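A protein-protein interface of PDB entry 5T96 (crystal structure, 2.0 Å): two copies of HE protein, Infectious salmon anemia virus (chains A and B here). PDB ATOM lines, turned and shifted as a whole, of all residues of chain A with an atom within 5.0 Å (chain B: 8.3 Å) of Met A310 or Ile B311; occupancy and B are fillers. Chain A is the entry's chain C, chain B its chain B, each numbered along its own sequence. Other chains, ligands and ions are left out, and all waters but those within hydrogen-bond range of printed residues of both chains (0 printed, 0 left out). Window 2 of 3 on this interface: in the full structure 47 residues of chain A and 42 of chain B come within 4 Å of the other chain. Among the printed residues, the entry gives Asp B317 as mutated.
NE2 of His A307 lies within hydrogen-bond range of O of Val B304 (3.2 Å). N of Lys B308 sits at hydrogen-bond distance from NE2 of His A307 (3.5 Å).
Among the printed residues, pairs that only touch across the chains: His A307 with His B307, His A307 with Ile B311, Met A310 with Ile B311, Ile A311 with Ile B311 and Leu A314 with Ile B318.
Met A310 touches one residue of chain B. Of the printed residues of chain A, Ile B311 touches His A307 (3.9 Å), Met A310 (3.8 Å) and Ile A311 (3.7 Å). No residue of chain B comes within 4 Å of Glu A309. Of the printed residues of chain B, Ile A311 touches Ile B311 (3.7 Å). Printed residues of chain A within 4 Å of Ile B318: Leu A314 (3.4 Å). Of the printed residues of chain A, Lys B308 touches His A307 (3.5 Å). The nearest printed residue of chain A that does not touch Val B304 is Met A310 (7.5 Å).
Hydrophobic or aromatic side chains of chain A that line the printed part of chain B: His A307, Met A310, Ile A311 and Leu A314. Printed residues of chain B that touch a printed residue of chain A: Val B304, His B307, Lys B308, Ile B311 and Ile B318. Among the printed residues, no Asp or Glu carboxylate lies within 4 Å of a Lys or Arg side-chain nitrogen of the other chain.
His A307 touches its own counterpart, His B307. His A307 touches Lys B308, but with the chains exchanged Lys A308 does not touch His B307 (8.3 Å). His A307 touches Ile B311, but with the chains exchanged Ile A311 does not touch His B307 (6.1 Å). Ile A311 touches its own counterpart, Ile B311. 9 positions are printed for both chains. Of the 7 pairs that touch across the chains among the printed residues, 2 have their exchanged pair printed and touching as well.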
ATOM      1  N   LEU A 306     -17.795   1.092   3.369  1.00  0.00           N
ATOM      2  CA  LEU A 306     -18.423  -0.225   3.326  1.00  0.00           C
ATOM      3  C   LEU A 306     -17.380  -1.330   3.456  1.00  0.00           C
ATOM      4  O   LEU A 306     -17.555  -2.283   4.225  1.00  0.00           O
ATOM      5  CB  LEU A 306     -19.217  -0.388   2.033  1.00  0.00           C
ATOM      6  CG  LEU A 306     -20.305   0.657   1.775  1.00  0.00           C
ATOM      7  CD1 LEU A 306     -21.011   0.374   0.455  1.00  0.00           C
ATOM      8  CD2 LEU A 306     -21.305   0.732   2.929  1.00  0.00           C
ATOM      9  N   HIS A 307     -16.270  -1.198   2.725  1.00  0.00           N
ATOM     10  CA  HIS A 307     -15.203  -2.192   2.795  1.00  0.00           C
ATOM     11  C   HIS A 307     -14.645  -2.304   4.211  1.00  0.00           C
ATOM     12  O   HIS A 307     -14.368  -3.409   4.692  1.00  0.00           O
ATOM     13  CB  HIS A 307     -14.095  -1.834   1.805  1.00  0.00           C
ATOM     14  CG  HIS A 307     -14.467  -2.056   0.369  1.00  0.00           C
ATOM     15  ND1 HIS A 307     -15.756  -2.312  -0.043  1.00  0.00           N
ATOM     16  CD2 HIS A 307     -13.704  -2.080  -0.747  1.00  0.00           C
ATOM     17  CE1 HIS A 307     -15.774  -2.465  -1.357  1.00  0.00           C
ATOM     18  NE2 HIS A 307     -14.540  -2.332  -1.807  1.00  0.00           N
ATOM     19  N   LYS A 308     -14.481  -1.172   4.896  1.00  0.00           N
ATOM     20  CA  LYS A 308     -14.060  -1.208   6.289  1.00  0.00           C
ATOM     21  C   LYS A 308     -15.026  -2.021   7.134  1.00  0.00           C
ATOM     22  O   LYS A 308     -14.603  -2.830   7.962  1.00  0.00           O
ATOM     23  CB  LYS A 308     -13.944   0.206   6.855  1.00  0.00           C
ATOM     24  CG  LYS A 308     -13.395   0.211   8.303  1.00  0.00           C
ATOM     25  CD  LYS A 308     -13.227   1.629   8.875  1.00  0.00           C
ATOM     26  CE  LYS A 308     -12.562   1.574  10.259  1.00  0.00           C
ATOM     27  NZ  LYS A 308     -12.797   2.810  11.092  1.00  0.00           N
ATOM     28  N   GLU A 309     -16.331  -1.812   6.947  1.00  0.00           N
ATOM     29  CA  GLU A 309     -17.315  -2.600   7.692  1.00  0.00           C
ATOM     30  C   GLU A 309     -17.219  -4.090   7.344  1.00  0.00           C
ATOM     31  O   GLU A 309     -17.243  -4.961   8.227  1.00  0.00           O
ATOM     32  CB  GLU A 309     -18.722  -2.065   7.401  1.00  0.00           C
ATOM     33  N   MET A 310     -17.117  -4.401   6.057  1.00  0.00           N
ATOM     34  CA  MET A 310     -17.074  -5.797   5.644  1.00  0.00           C
ATOM     35  C   MET A 310     -15.798  -6.465   6.126  1.00  0.00           C
ATOM     36  O   MET A 310     -15.808  -7.650   6.463  1.00  0.00           O
ATOM     37  CB  MET A 310     -17.180  -5.905   4.124  1.00  0.00           C
ATOM     38  CG  MET A 310     -18.423  -5.269   3.538  1.00  0.00           C
ATOM     39  SD  MET A 310     -18.625  -5.622   1.782  1.00  0.00           S
ATOM     40  CE  MET A 310     -17.319  -4.644   1.081  1.00  0.00           C
ATOM     41  N   ILE A 311     -14.679  -5.733   6.135  1.00  0.00           N
ATOM     42  CA  ILE A 311     -13.434  -6.308   6.638  1.00  0.00           C
ATOM     43  C   ILE A 311     -13.544  -6.574   8.133  1.00  0.00           C
ATOM     44  O   ILE A 311     -13.075  -7.605   8.640  1.00  0.00           O
ATOM     45  CB  ILE A 311     -12.242  -5.389   6.322  1.00  0.00           C
ATOM     46  CG1 ILE A 311     -11.939  -5.398   4.818  1.00  0.00           C
ATOM     47  CG2 ILE A 311     -10.979  -5.831   7.134  1.00  0.00           C
ATOM     48  CD1 ILE A 311     -10.901  -4.318   4.396  1.00  0.00           C
ATOM     49  N   SER A 312     -14.162  -5.651   8.863  1.00  0.00           N
ATOM     50  CA  SER A 312     -14.387  -5.869  10.285  1.00  0.00           C
ATOM     51  C   SER A 312     -15.177  -7.149  10.541  1.00  0.00           C
ATOM     52  O   SER A 312     -14.806  -7.958  11.402  1.00  0.00           O
ATOM     53  CB  SER A 312     -15.099  -4.658  10.870  1.00  0.00           C
ATOM     54  OG  SER A 312     -14.279  -3.515  10.707  1.00  0.00           O
ATOM     55  N   LYS A 313     -16.288  -7.340   9.823  1.00  0.00           N
ATOM     56  CA  LYS A 313     -17.069  -8.568   9.980  1.00  0.00           C
ATOM     57  C   LYS A 313     -16.224  -9.802   9.662  1.00  0.00           C
ATOM     58  O   LYS A 313     -16.268 -10.803  10.384  1.00  0.00           O
ATOM     59  CB  LYS A 313     -18.313  -8.519   9.089  1.00  0.00           C
ATOM     60  N   LEU A 314     -15.481  -9.762   8.549  1.00  0.00           N
ATOM     61  CA  LEU A 314     -14.563 -10.852   8.217  1.00  0.00           C
ATOM     62  C   LEU A 314     -13.615 -11.156   9.384  1.00  0.00           C
ATOM     63  O   LEU A 314     -13.376 -12.326   9.719  1.00  0.00           O
ATOM     64  CB  LEU A 314     -13.784 -10.496   6.949  1.00  0.00           C
ATOM     65  N   VAL B 304     -10.143  -0.330  -5.447  1.00  0.00           N
ATOM     66  CA  VAL B 304     -11.304  -0.572  -4.594  1.00  0.00           C
ATOM     67  C   VAL B 304     -12.230  -1.620  -5.208  1.00  0.00           C
ATOM     68  O   VAL B 304     -12.793  -2.464  -4.496  1.00  0.00           O
ATOM     69  CB  VAL B 304     -12.033   0.760  -4.337  1.00  0.00           C
ATOM     70  CG1 VAL B 304     -13.415   0.530  -3.743  1.00  0.00           C
ATOM     71  CG2 VAL B 304     -11.202   1.603  -3.397  1.00  0.00           C
ATOM     72  N   ALA B 305     -12.434  -1.564  -6.527  1.00  0.00           N
ATOM     73  CA  ALA B 305     -13.227  -2.591  -7.197  1.00  0.00           C
ATOM     74  C   ALA B 305     -12.631  -3.973  -6.966  1.00  0.00           C
ATOM     75  O   ALA B 305     -13.352  -4.933  -6.658  1.00  0.00           O
ATOM     76  CB  ALA B 305     -13.320  -2.292  -8.694  1.00  0.00           C
ATOM     77  N   LEU B 306     -11.311  -4.095  -7.111  1.00  0.00           N
ATOM     78  CA  LEU B 306     -10.659  -5.361  -6.813  1.00  0.00           C
ATOM     79  C   LEU B 306     -10.959  -5.796  -5.386  1.00  0.00           C
ATOM     80  O   LEU B 306     -11.305  -6.959  -5.136  1.00  0.00           O
ATOM     81  CB  LEU B 306      -9.152  -5.242  -7.050  1.00  0.00           C
ATOM     82  CG  LEU B 306      -8.619  -5.256  -8.500  1.00  0.00           C
ATOM     83  CD1 LEU B 306      -7.072  -5.255  -8.516  1.00  0.00           C
ATOM     84  CD2 LEU B 306      -9.148  -6.452  -9.329  1.00  0.00           C
ATOM     85  N   HIS B 307     -10.868  -4.859  -4.440  1.00  0.00           N
ATOM     86  CA  HIS B 307     -11.111  -5.163  -3.031  1.00  0.00           C
ATOM     87  C   HIS B 307     -12.511  -5.711  -2.808  1.00  0.00           C
ATOM     88  O   HIS B 307     -12.700  -6.623  -1.995  1.00  0.00           O
ATOM     89  CB  HIS B 307     -10.900  -3.911  -2.167  1.00  0.00           C
ATOM     90  CG  HIS B 307      -9.458  -3.532  -1.952  1.00  0.00           C
ATOM     91  ND1 HIS B 307      -8.408  -4.114  -2.635  1.00  0.00           N
ATOM     92  CD2 HIS B 307      -8.900  -2.627  -1.112  1.00  0.00           C
ATOM     93  CE1 HIS B 307      -7.270  -3.571  -2.236  1.00  0.00           C
ATOM     94  NE2 HIS B 307      -7.543  -2.659  -1.319  1.00  0.00           N
ATOM     95  N   LYS B 308     -13.513  -5.170  -3.513  1.00  0.00           N
ATOM     96  CA  LYS B 308     -14.883  -5.638  -3.311  1.00  0.00           C
ATOM     97  C   LYS B 308     -14.985  -7.138  -3.548  1.00  0.00           C
ATOM     98  O   LYS B 308     -15.614  -7.865  -2.765  1.00  0.00           O
ATOM     99  CB  LYS B 308     -15.854  -4.897  -4.231  1.00  0.00           C
ATOM    100  CG  LYS B 308     -17.313  -5.327  -4.054  1.00  0.00           C
ATOM    101  CD  LYS B 308     -18.292  -4.435  -4.812  1.00  0.00           C
ATOM    102  CE  LYS B 308     -18.256  -4.678  -6.309  1.00  0.00           C
ATOM    103  NZ  LYS B 308     -18.914  -3.568  -7.059  1.00  0.00           N
ATOM    104  N   GLU B 309     -14.360  -7.624  -4.618  1.00  0.00           N
ATOM    105  CA  GLU B 309     -14.440  -9.046  -4.940  1.00  0.00           C
ATOM    106  C   GLU B 309     -13.484  -9.883  -4.103  1.00  0.00           C
ATOM    107  O   GLU B 309     -13.813 -11.026  -3.767  1.00  0.00           O
ATOM    108  CB  GLU B 309     -14.171  -9.264  -6.430  1.00  0.00           C
ATOM    109  CG  GLU B 309     -15.300  -8.759  -7.327  1.00  0.00           C
ATOM    110  CD  GLU B 309     -16.618  -9.501  -7.105  1.00  0.00           C
ATOM    111  OE1 GLU B 309     -16.587 -10.702  -6.758  1.00  0.00           O
ATOM    112  OE2 GLU B 309     -17.688  -8.877  -7.272  1.00  0.00           O
ATOM    113  N   MET B 310     -12.302  -9.352  -3.767  1.00  0.00           N
ATOM    114  CA  MET B 310     -11.437 -10.047  -2.814  1.00  0.00           C
ATOM    115  C   MET B 310     -12.153 -10.266  -1.494  1.00  0.00           C
ATOM    116  O   MET B 310     -12.083 -11.353  -0.908  1.00  0.00           O
ATOM    117  CB  MET B 310     -10.162  -9.257  -2.569  1.00  0.00           C
ATOM    118  CG  MET B 310      -9.015  -9.646  -3.445  1.00  0.00           C
ATOM    119  SD  MET B 310      -7.610  -8.573  -3.156  1.00  0.00           S
ATOM    120  CE  MET B 310      -8.207  -7.078  -3.911  1.00  0.00           C
ATOM    121  N   ILE B 311     -12.837  -9.239  -1.002  1.00  0.00           N
ATOM    122  CA  ILE B 311     -13.596  -9.374   0.236  1.00  0.00           C
ATOM    123  C   ILE B 311     -14.706 -10.402   0.068  1.00  0.00           C
ATOM    124  O   ILE B 311     -14.915 -11.261   0.935  1.00  0.00           O
ATOM    125  CB  ILE B 311     -14.137  -8.004   0.669  1.00  0.00           C
ATOM    126  CG1 ILE B 311     -12.963  -7.141   1.137  1.00  0.00           C
ATOM    127  CG2 ILE B 311     -15.171  -8.131   1.767  1.00  0.00           C
ATOM    128  CD1 ILE B 311     -13.317  -5.671   1.368  1.00  0.00           C
ATOM    129  N   SER B 312     -15.441 -10.325  -1.044  1.00  0.00           N
ATOM    130  CA  SER B 312     -16.484 -11.309  -1.315  1.00  0.00           C
ATOM    131  C   SER B 312     -15.948 -12.743  -1.231  1.00  0.00           C
ATOM    132  O   SER B 312     -16.598 -13.624  -0.654  1.00  0.00           O
ATOM    133  CB  SER B 312     -17.101 -11.034  -2.691  1.00  0.00           C
ATOM    134  N   LYS B 313     -14.758 -12.995  -1.788  1.00  0.00           N
ATOM    135  CA  LYS B 313     -14.226 -14.355  -1.793  1.00  0.00           C
ATOM    136  C   LYS B 313     -13.806 -14.784  -0.393  1.00  0.00           C
ATOM    137  O   LYS B 313     -14.004 -15.940  -0.011  1.00  0.00           O
ATOM    138  CB  LYS B 313     -13.048 -14.465  -2.764  1.00  0.00           C
ATOM    139  N   LEU B 314     -13.235 -13.869   0.394  1.00  0.00           N
ATOM    140  CA  LEU B 314     -12.898 -14.216   1.769  1.00  0.00           C
ATOM    141  C   LEU B 314     -14.154 -14.494   2.594  1.00  0.00           C
ATOM    142  O   LEU B 314     -14.145 -15.408   3.436  1.00  0.00           O
ATOM    143  CB  LEU B 314     -12.043 -13.117   2.409  1.00  0.00           C
ATOM    144  CG  LEU B 314     -10.536 -13.287   2.162  1.00  0.00           C
ATOM    145  CD1 LEU B 314     -10.234 -13.475   0.683  1.00  0.00           C
ATOM    146  CD2 LEU B 314      -9.727 -12.114   2.697  1.00  0.00           C
ATOM    147  N   GLN B 315     -15.254 -13.771   2.335  1.00  0.00           N
ATOM    148  CA  GLN B 315     -16.498 -14.050   3.058  1.00  0.00           C
ATOM    149  C   GLN B 315     -16.993 -15.465   2.781  1.00  0.00           C
ATOM    150  O   GLN B 315     -17.446 -16.163   3.693  1.00  0.00           O
ATOM    151  CB  GLN B 315     -17.582 -13.036   2.693  1.00  0.00           C
ATOM    152  N   ARG B 316     -16.941 -15.899   1.527  1.00  0.00           N
ATOM    153  CA  ARG B 316     -17.364 -17.258   1.220  1.00  0.00           C
ATOM    154  C   ARG B 316     -16.397 -18.283   1.807  1.00  0.00           C
ATOM    155  O   ARG B 316     -16.829 -19.334   2.299  1.00  0.00           O
ATOM    156  CB  ARG B 316     -17.498 -17.428  -0.290  1.00  0.00           C
ATOM    157  CG  ARG B 316     -18.538 -16.513  -0.907  1.00  0.00           C
ATOM    158  CD  ARG B 316     -18.787 -16.855  -2.371  1.00  0.00           C
ATOM    159  NE  ARG B 316     -17.591 -16.692  -3.202  1.00  0.00           N
ATOM    160  CZ  ARG B 316     -17.258 -15.576  -3.848  1.00  0.00           C
ATOM    161  NH1 ARG B 316     -18.027 -14.497  -3.773  1.00  0.00           N
ATOM    162  NH2 ARG B 316     -16.150 -15.538  -4.575  1.00  0.00           N
ATOM    163  N   ASP B 317     -15.091 -17.993   1.780  1.00  0.00           N
ATOM    164  CA  ASP B 317     -14.108 -18.911   2.359  1.00  0.00           C
ATOM    165  C   ASP B 317     -14.330 -19.094   3.863  1.00  0.00           C
ATOM    166  O   ASP B 317     -14.339 -20.225   4.363  1.00  0.00           O
ATOM    167  CB  ASP B 317     -12.686 -18.417   2.077  1.00  0.00           C
ATOM    168  CG  ASP B 317     -12.310 -18.497   0.582  1.00  0.00           C
ATOM    169  OD1 ASP B 317     -13.041 -19.150  -0.195  1.00  0.00           O
ATOM    170  OD2 ASP B 317     -11.276 -17.909   0.187  1.00  0.00           O
ATOM    171  N   ILE B 318     -14.508 -17.992   4.603  1.00  0.00           N
ATOM    172  CA  ILE B 318     -14.803 -18.096   6.035  1.00  0.00           C
ATOM    173  C   ILE B 318     -16.049 -18.944   6.254  1.00  0.00           C
ATOM    174  O   ILE B 318     -16.043 -19.900   7.037  1.00  0.00           O
ATOM    175  CB  ILE B 318     -14.969 -16.699   6.671  1.00  0.00           C
ATOM    176  CG1 ILE B 318     -13.663 -15.921   6.619  1.00  0.00           C
ATOM    177  CG2 ILE B 318     -15.413 -16.819   8.121  1.00  0.00           C
ATOM    178  CD1 ILE B 318     -13.782 -14.465   7.067  1.00  0.00           C
